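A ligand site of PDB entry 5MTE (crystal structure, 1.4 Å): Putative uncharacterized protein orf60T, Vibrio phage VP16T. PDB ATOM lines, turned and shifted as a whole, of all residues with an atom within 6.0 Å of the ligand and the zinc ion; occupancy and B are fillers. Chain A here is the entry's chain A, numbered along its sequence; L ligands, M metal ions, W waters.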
ATOM      1  N   ALA A  38       8.504  14.185   5.437  1.00  0.00           N
ATOM      2  CA  ALA A  38       9.330  12.970   5.368  1.00  0.00           C
ATOM      3  C   ALA A  38      10.496  13.079   4.376  1.00  0.00           C
ATOM      4  O   ALA A  38      11.303  12.152   4.251  1.00  0.00           O
ATOM      5  CB  ALA A  38       8.471  11.771   5.038  1.00  0.00           C
ATOM      6  N   GLY A  39      10.577  14.202   3.665  1.00  0.00           N
ATOM      7  CA  GLY A  39      11.674  14.453   2.730  1.00  0.00           C
ATOM      8  C   GLY A  39      11.556  13.724   1.412  1.00  0.00           C
ATOM      9  O   GLY A  39      12.570  13.379   0.790  1.00  0.00           O
ATOM     10  N   GLY A  40      10.334  13.490   0.960  1.00  0.00           N
ATOM     11  CA  GLY A  40      10.126  12.771  -0.292  1.00  0.00           C
ATOM     12  C   GLY A  40       9.853  13.685  -1.474  1.00  0.00           C
ATOM     13  O   GLY A  40       9.594  14.879  -1.282  1.00  0.00           O
ATOM     14  N   ILE A  41       9.970  13.130  -2.681  1.00  0.00           N
ATOM     15  CA  ILE A  41       9.608  13.874  -3.910  1.00  0.00           C
ATOM     16  C   ILE A  41       8.306  13.366  -4.534  1.00  0.00           C
ATOM     17  O   ILE A  41       7.855  13.872  -5.553  1.00  0.00           O
ATOM     18  CB  ILE A  41      10.755  13.904  -4.955  1.00  0.00           C
ATOM     19  CG1 ILE A  41      11.128  12.494  -5.409  1.00  0.00           C
ATOM     20  CG2 ILE A  41      11.960  14.651  -4.394  1.00  0.00           C
ATOM     21  CD1 ILE A  41      12.132  12.455  -6.554  1.00  0.00           C
ATOM     22  N   GLY A  42       7.687  12.384  -3.882  1.00  0.00           N
ATOM     23  CA  GLY A  42       6.369  11.884  -4.268  1.00  0.00           C
ATOM     24  C   GLY A  42       5.753  11.158  -3.098  1.00  0.00           C
ATOM     25  O   GLY A  42       6.437  10.816  -2.149  1.00  0.00           O
ATOM     26  N   LEU A  43       4.431  10.951  -3.179  1.00  0.00           N
ATOM     27  CA  LEU A  43       3.717  10.166  -2.181  1.00  0.00           C
ATOM     28  C   LEU A  43       2.418   9.684  -2.788  1.00  0.00           C
ATOM     29  O   LEU A  43       1.835  10.365  -3.630  1.00  0.00           O
ATOM     30  CB  LEU A  43       3.462  10.997  -0.914  1.00  0.00           C
ATOM     31  CG  LEU A  43       3.111  10.217   0.356  1.00  0.00           C
ATOM     32  CD1 LEU A  43       4.380   9.562   0.908  1.00  0.00           C
ATOM     33  CD2 LEU A  43       2.522  11.138   1.420  1.00  0.00           C
ATOM     34  N   ALA A  44       1.977   8.510  -2.348  1.00  0.00           N
ATOM     35  CA  ALA A  44       0.735   7.909  -2.812  1.00  0.00           C
ATOM     36  C   ALA A  44      -0.188   7.665  -1.626  1.00  0.00           C
ATOM     37  O   ALA A  44       0.281   7.435  -0.502  1.00  0.00           O
ATOM     38  CB  ALA A  44       1.034   6.577  -3.497  1.00  0.00           C
ATOM     39  N   GLN A  47       0.406   5.086   1.214  1.00  0.00           N
ATOM     40  CA  GLN A  47       1.509   5.277   2.175  1.00  0.00           C
ATOM     41  C   GLN A  47       1.100   5.974   3.451  1.00  0.00           C
ATOM     42  O   GLN A  47       1.812   5.893   4.464  1.00  0.00           O
ATOM     43  CB  GLN A  47       2.648   6.051   1.542  1.00  0.00           C
ATOM     44  CG  GLN A  47       3.331   5.312   0.424  1.00  0.00           C
ATOM     45  CD  GLN A  47       4.402   6.173  -0.195  1.00  0.00           C
ATOM     46  OE1 GLN A  47       4.117   7.051  -1.010  1.00  0.00           O
ATOM     47  NE2 GLN A  47       5.652   5.944   0.205  1.00  0.00           N
ATOM     48  N   SER A  81      16.835   2.917 -12.715  1.00  0.00           N
ATOM     49  CA  SER A  81      16.377   3.955 -11.805  1.00  0.00           C
ATOM     50  C   SER A  81      16.642   3.558 -10.344  1.00  0.00           C
ATOM     51  O   SER A  81      15.915   2.742  -9.806  1.00  0.00           O
ATOM     52  CB  SER A  81      14.876   4.176 -12.001  1.00  0.00           C
ATOM     53  OG  SER A  81      14.330   5.047 -11.011  1.00  0.00           O
ATOM     54  N   PRO A  82      17.667   4.151  -9.700  1.00  0.00           N
ATOM     55  CA  PRO A  82      17.903   3.811  -8.286  1.00  0.00           C
ATOM     56  C   PRO A  82      16.886   4.536  -7.403  1.00  0.00           C
ATOM     57  O   PRO A  82      16.775   5.761  -7.474  1.00  0.00           O
ATOM     58  CB  PRO A  82      19.336   4.288  -8.047  1.00  0.00           C
ATOM     59  CG  PRO A  82      19.535   5.424  -9.043  1.00  0.00           C
ATOM     60  CD  PRO A  82      18.655   5.129 -10.218  1.00  0.00           C
ATOM     61  N   GLU A  83      16.156   3.778  -6.580  1.00  0.00           N
ATOM     62  CA  GLU A  83      15.051   4.364  -5.831  1.00  0.00           C
ATOM     63  C   GLU A  83      15.050   3.933  -4.384  1.00  0.00           C
ATOM     64  O   GLU A  83      15.283   2.755  -4.086  1.00  0.00           O
ATOM     65  CB  GLU A  83      13.722   3.947  -6.463  1.00  0.00           C
ATOM     66  CG  GLU A  83      13.606   4.343  -7.932  1.00  0.00           C
ATOM     67  CD  GLU A  83      12.288   3.968  -8.563  1.00  0.00           C
ATOM     68  OE1 GLU A  83      11.344   3.614  -7.816  1.00  0.00           O
ATOM     69  OE2 GLU A  83      12.192   4.040  -9.816  1.00  0.00           O
ATOM     70  N   GLY A  84      14.796   4.888  -3.499  1.00  0.00           N
ATOM     71  CA  GLY A  84      14.400   4.582  -2.146  1.00  0.00           C
ATOM     72  C   GLY A  84      12.925   4.913  -2.018  1.00  0.00           C
ATOM     73  O   GLY A  84      12.325   5.564  -2.902  1.00  0.00           O
ATOM     74  N   CYS A  85      12.329   4.478  -0.917  1.00  0.00           N
ATOM     75  CA  CYS A  85      10.917   4.674  -0.668  1.00  0.00           C
ATOM     76  C   CYS A  85      10.727   5.119   0.759  1.00  0.00           C
ATOM     77  O   CYS A  85      11.345   4.550   1.655  1.00  0.00           O
ATOM     78  CB  CYS A  85      10.147   3.373  -0.937  1.00  0.00           C
ATOM     79  SG  CYS A  85       8.331   3.518  -0.707  1.00  0.00           S
ATOM     80  N   LEU A  86       9.871   6.115   0.973  1.00  0.00           N
ATOM     81  CA  LEU A  86       9.626   6.614   2.326  1.00  0.00           C
ATOM     82  C   LEU A  86       9.005   5.563   3.236  1.00  0.00           C
ATOM     83  O   LEU A  86       9.118   5.670   4.448  1.00  0.00           O
ATOM     84  CB  LEU A  86       8.701   7.834   2.290  1.00  0.00           C
ATOM     85  CG  LEU A  86       9.252   9.104   1.654  1.00  0.00           C
ATOM     86  CD1 LEU A  86       8.141  10.158   1.666  1.00  0.00           C
ATOM     87  CD2 LEU A  86      10.485   9.560   2.388  1.00  0.00           C
ATOM     88  N   SER A  87       8.360   4.566   2.652  1.00  0.00           N
ATOM     89  CA  SER A  87       7.746   3.493   3.442  1.00  0.00           C
ATOM     90  C   SER A  87       8.769   2.445   3.874  1.00  0.00           C
ATOM     91  O   SER A  87       8.467   1.688   4.793  1.00  0.00           O
ATOM     92  CB  SER A  87       6.632   2.833   2.649  1.00  0.00           C
ATOM     93  OG  SER A  87       5.652   3.794   2.313  1.00  0.00           O
ATOM     94  N   LYS A  91      16.574   1.487   2.426  1.00  0.00           N
ATOM     95  CA  LYS A  91      16.702   0.567   1.289  1.00  0.00           C
ATOM     96  C   LYS A  91      16.804   1.404   0.007  1.00  0.00           C
ATOM     97  O   LYS A  91      15.986   2.279  -0.196  1.00  0.00           O
ATOM     98  CB  LYS A  91      15.416  -0.316   1.215  1.00  0.00           C
ATOM     99  CG  LYS A  91      15.361  -1.389   0.130  1.00  0.00           C
ATOM    100  CD  LYS A  91      13.909  -1.784  -0.263  1.00  0.00           C
ATOM    101  CE  LYS A  91      13.350  -2.887   0.596  1.00  0.00           C
ATOM    102  NZ  LYS A  91      12.397  -3.668  -0.240  1.00  0.00           N
ATOM    103  N   THR A  92      17.794   1.109  -0.840  1.00  0.00           N
ATOM    104  CA  THR A  92      17.778   1.631  -2.218  1.00  0.00           C
ATOM    105  C   THR A  92      17.802   0.455  -3.183  1.00  0.00           C
ATOM    106  O   THR A  92      18.612  -0.469  -3.013  1.00  0.00           O
ATOM    107  CB  THR A  92      18.974   2.568  -2.499  1.00  0.00           C
ATOM    108  OG1 THR A  92      19.006   3.586  -1.493  1.00  0.00           O
ATOM    109  CG2 THR A  92      18.853   3.190  -3.889  1.00  0.00           C
ATOM    110  N   LEU A 120      13.867  11.200 -14.204  1.00  0.00           N
ATOM    111  CA  LEU A 120      13.452  11.163 -12.807  1.00  0.00           C
ATOM    112  C   LEU A 120      11.948  11.377 -12.607  1.00  0.00           C
ATOM    113  O   LEU A 120      11.317  10.639 -11.852  1.00  0.00           O
ATOM    114  CB  LEU A 120      14.253  12.156 -11.969  1.00  0.00           C
ATOM    115  CG  LEU A 120      13.921  12.164 -10.470  1.00  0.00           C
ATOM    116  CD1 LEU A 120      14.067  10.797  -9.813  1.00  0.00           C
ATOM    117  CD2 LEU A 120      14.785  13.206  -9.754  1.00  0.00           C
ATOM    118  N   PHE A 123      10.151   8.373 -13.563  1.00  0.00           N
ATOM    119  CA  PHE A 123      10.392   7.335 -12.562  1.00  0.00           C
ATOM    120  C   PHE A 123       9.485   7.561 -11.355  1.00  0.00           C
ATOM    121  O   PHE A 123       8.891   6.616 -10.836  1.00  0.00           O
ATOM    122  CB  PHE A 123      11.861   7.332 -12.095  1.00  0.00           C
ATOM    123  CG  PHE A 123      12.874   7.179 -13.211  1.00  0.00           C
ATOM    124  CD1 PHE A 123      14.187   7.596 -13.012  1.00  0.00           C
ATOM    125  CD2 PHE A 123      12.521   6.603 -14.433  1.00  0.00           C
ATOM    126  CE1 PHE A 123      15.134   7.451 -14.025  1.00  0.00           C
ATOM    127  CE2 PHE A 123      13.468   6.471 -15.464  1.00  0.00           C
ATOM    128  CZ  PHE A 123      14.781   6.899 -15.253  1.00  0.00           C
ATOM    129  N   CYS A 124       9.398   8.819 -10.900  1.00  0.00           N
ATOM    130  CA  CYS A 124       8.534   9.135  -9.758  1.00  0.00           C
ATOM    131  C   CYS A 124       7.078   8.752 -10.023  1.00  0.00           C
ATOM    132  O   CYS A 124       6.419   8.132  -9.185  1.00  0.00           O
ATOM    133  CB  CYS A 124       8.521  10.627  -9.424  1.00  0.00           C
ATOM    134  SG  CYS A 124      10.043  11.575  -9.199  1.00  0.00           S
ATOM    135  N   LEU A 125       6.554   9.176 -11.180  1.00  0.00           N
ATOM    136  CA  LEU A 125       5.182   8.828 -11.534  1.00  0.00           C
ATOM    137  C   LEU A 125       4.945   7.328 -11.496  1.00  0.00           C
ATOM    138  O   LEU A 125       3.938   6.857 -10.956  1.00  0.00           O
ATOM    139  CB  LEU A 125       4.821   9.394 -12.907  1.00  0.00           C
ATOM    140  CG  LEU A 125       4.640  10.912 -12.899  1.00  0.00           C
ATOM    141  CD1 LEU A 125       4.758  11.509 -14.303  1.00  0.00           C
ATOM    142  CD2 LEU A 125       3.308  11.318 -12.272  1.00  0.00           C
ATOM    143  N   HIS A 127       6.675   5.089  -9.814  1.00  0.00           N
ATOM    144  CA  HIS A 127       6.830   4.663  -8.405  1.00  0.00           C
ATOM    145  C   HIS A 127       5.523   4.886  -7.644  1.00  0.00           C
ATOM    146  O   HIS A 127       5.056   3.993  -6.918  1.00  0.00           O
ATOM    147  CB  HIS A 127       7.990   5.449  -7.783  1.00  0.00           C
ATOM    148  CG  HIS A 127       8.284   5.119  -6.342  1.00  0.00           C
ATOM    149  ND1 HIS A 127       9.443   4.489  -5.936  1.00  0.00           N
ATOM    150  CD2 HIS A 127       7.595   5.392  -5.211  1.00  0.00           C
ATOM    151  CE1 HIS A 127       9.441   4.363  -4.622  1.00  0.00           C
ATOM    152  NE2 HIS A 127       8.327   4.906  -4.157  1.00  0.00           N
ATOM    153  N   GLU A 128       4.916   6.069  -7.826  1.00  0.00           N
ATOM    154  CA  GLU A 128       3.693   6.403  -7.075  1.00  0.00           C
ATOM    155  C   GLU A 128       2.480   5.611  -7.574  1.00  0.00           C
ATOM    156  O   GLU A 128       1.649   5.157  -6.771  1.00  0.00           O
ATOM    157  CB  GLU A 128       3.383   7.903  -7.121  1.00  0.00           C
ATOM    158  CG  GLU A 128       4.494   8.845  -6.623  1.00  0.00           C
ATOM    159  CD  GLU A 128       5.166   8.407  -5.309  1.00  0.00           C
ATOM    160  OE1 GLU A 128       4.540   7.669  -4.501  1.00  0.00           O
ATOM    161  OE2 GLU A 128       6.319   8.842  -5.101  1.00  0.00           O
ATOM    162  N   HIS A 131       2.507   2.229  -6.138  1.00  0.00           N
ATOM    163  CA  HIS A 131       1.978   2.182  -4.779  1.00  0.00           C
ATOM    164  C   HIS A 131       0.465   1.979  -4.777  1.00  0.00           C
ATOM    165  O   HIS A 131      -0.055   1.245  -3.933  1.00  0.00           O
ATOM    166  CB  HIS A 131       2.257   3.467  -3.995  1.00  0.00           C
ATOM    167  CG  HIS A 131       3.591   3.517  -3.306  1.00  0.00           C
ATOM    168  ND1 HIS A 131       3.928   2.666  -2.274  1.00  0.00           N
ATOM    169  CD2 HIS A 131       4.651   4.336  -3.485  1.00  0.00           C
ATOM    170  CE1 HIS A 131       5.143   2.969  -1.850  1.00  0.00           C
ATOM    171  NE2 HIS A 131       5.595   3.982  -2.564  1.00  0.00           N
ATOM    172  N   ILE A 137       8.921  -1.154  -4.017  1.00  0.00           N
ATOM    173  CA  ILE A 137      10.289  -1.443  -4.495  1.00  0.00           C
ATOM    174  C   ILE A 137      10.921  -2.661  -3.811  1.00  0.00           C
ATOM    175  O   ILE A 137      10.645  -2.936  -2.644  1.00  0.00           O
ATOM    176  CB  ILE A 137      11.215  -0.196  -4.401  1.00  0.00           C
ATOM    177  CG1 ILE A 137      11.447   0.215  -2.938  1.00  0.00           C
ATOM    178  CG2 ILE A 137      10.659   0.988  -5.242  1.00  0.00           C
ATOM    179  CD1 ILE A 137      12.554   1.273  -2.761  1.00  0.00           C
ATOM    180  OXT ILE A 137      11.771  -3.318  -4.476  1.00  0.00           O
HETATM  181  C1  LIG L   1       9.149   8.853  -2.050  1.00  0.00           C
HETATM  182  C2  LIG L   1       8.210   7.670  -2.007  1.00  0.00           C
HETATM  183  O1  LIG L   1       8.409   6.677  -1.309  1.00  0.00           O
HETATM  184  N1  LIG L   1       7.156   7.770  -2.810  1.00  0.00           N
HETATM  185  O2  LIG L   1       6.294   6.734  -2.822  1.00  0.00           O
HETATM  186  C3  LIG L   1      10.326   8.515  -2.970  1.00  0.00           C
HETATM  187  C4  LIG L   1      11.533   9.406  -2.723  1.00  0.00           C
HETATM  188  O3  LIG L   1      11.426  10.624  -2.523  1.00  0.00           O
HETATM  189  C5  LIG L   1       9.909   8.688  -4.451  1.00  0.00           C
HETATM  190  C6  LIG L   1      10.969   8.112  -5.397  1.00  0.00           C
HETATM  191  C7  LIG L   1      10.532   8.188  -6.863  1.00  0.00           C
HETATM  192  C8  LIG L   1      11.569   7.576  -7.821  1.00  0.00           C
HETATM  193  C9  LIG L   1      12.980   8.056  -7.492  1.00  0.00           C
HETATM  194  N2  LIG L   1      12.677   8.731  -2.780  1.00  0.00           N
HETATM  195  C10 LIG L   1      13.993   9.358  -2.672  1.00  0.00           C
HETATM  196  C11 LIG L   1      14.733   9.080  -1.339  1.00  0.00           C
HETATM  197  C12 LIG L   1      13.916   9.515  -0.118  1.00  0.00           C
HETATM  198  C13 LIG L   1      15.140   7.632  -1.176  1.00  0.00           C
HETATM  199  C14 LIG L   1      14.768   8.864  -3.915  1.00  0.00           C
HETATM  200  O4  LIG L   1      14.730   7.673  -4.268  1.00  0.00           O
HETATM  201  N3  LIG L   1      15.461   9.713  -4.684  1.00  0.00           N
HETATM  202  C15 LIG L   1      16.204   9.290  -5.888  1.00  0.00           C
HETATM  203  C16 LIG L   1      15.577  11.162  -4.436  1.00  0.00           C
HETATM  204  C17 LIG L   1      16.583  11.648  -5.476  1.00  0.00           C
HETATM  205  C18 LIG L   1      16.486  10.610  -6.605  1.00  0.00           C
HETATM  206  C19 LIG L   1      17.505   8.583  -5.477  1.00  0.00           C
HETATM  207  O5  LIG L   1      18.080   7.931  -6.611  1.00  0.00           O
HETATM  208 ZN    ZN M   1       7.453   4.981  -2.273  1.00  0.00          ZN
HETATM  209  O   HOH W   1      17.638   5.895  -1.297  1.00  0.00           O
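The side-chain carboxylate of Glu 128 is in hydrogen-bond range of a nitrogen (N1) of the ligand. O3 of the ligand sits at hydrogen-bond distance from N of Ile 41 (2.9 Å). N of Gly 84 sits at hydrogen-bond distance from O4 of the ligand (2.9 Å). The side-chain amide oxygen (OE1) of Gln 47 lies close to an oxygen (O2) of the ligand (2.9 Å). The backbone carbonyl oxygen (O) of Gly 42 sits at hydrogen-bond distance from a nitrogen (N1) of the ligand. A nitrogen (N2) of the ligand is in hydrogen-bond range of the backbone carbonyl oxygen of Gly 84, 3.2 Å away. N of Leu 86 sits close to O1 of the ligand (2.8 Å). O5 of the ligand sits at hydrogen-bond distance from O of Pro 82.
The backbone NH (N) of Ala 44 is in hydrogen-bond range of the side-chain amide oxygen (OE1) of Gln 47, 2.9 Å away. The side-chain amide nitrogen (NE2) of Gln 47 sits close to a ring nitrogen (NE2) of His 131 (3.4 Å). OE1 of Glu 128 is in hydrogen-bond range of N of Ala 44. NE2 of Gln 47 is in hydrogen-bond range of OG of Ser 87 (3.0 Å). ND1 of His 127 sits at hydrogen-bond distance from OE1 of Glu 83. The side-chain sulfur (SG) of Cys 85 sits close to the backbone NH (N) of Ser 87, 3.5 Å away. The side-chain carboxylate (OE2) of Glu 128 lies close to the backbone NH (N) of Leu 43, at 3.4 Å. The side-chain carboxylate (OE2) of Glu 83 sits at hydrogen-bond distance from the side-chain hydroxyl (OG) of Ser 81 (2.6 Å).
Residues that only touch the ligand: Gly 40 (3.4 Å), Glu 83 (3.7 Å), Leu 120 (3.8 Å) and Cys 124 (3.6 Å).
Gln 47 touches the zinc ion (NE2 to ZN, 3.2 Å). Four residues have an atom within 4 Å of the zinc ion: Gln 47, Cys 85, His 127 and His 131. The nearest printed residue that does not touch the zinc ion is Leu 86 (4.2 Å).
The zinc ion is bound by a ring nitrogen (NE2) of His 127 (2.1 Å), a ring nitrogen (NE2) of His 131 (2.1 Å), an oxygen (O2) of the ligand (2.2 Å), an oxygen (O1) of the ligand (2.2 Å) and the side-chain sulfur (SG) of Cys 85 (2.3 Å).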
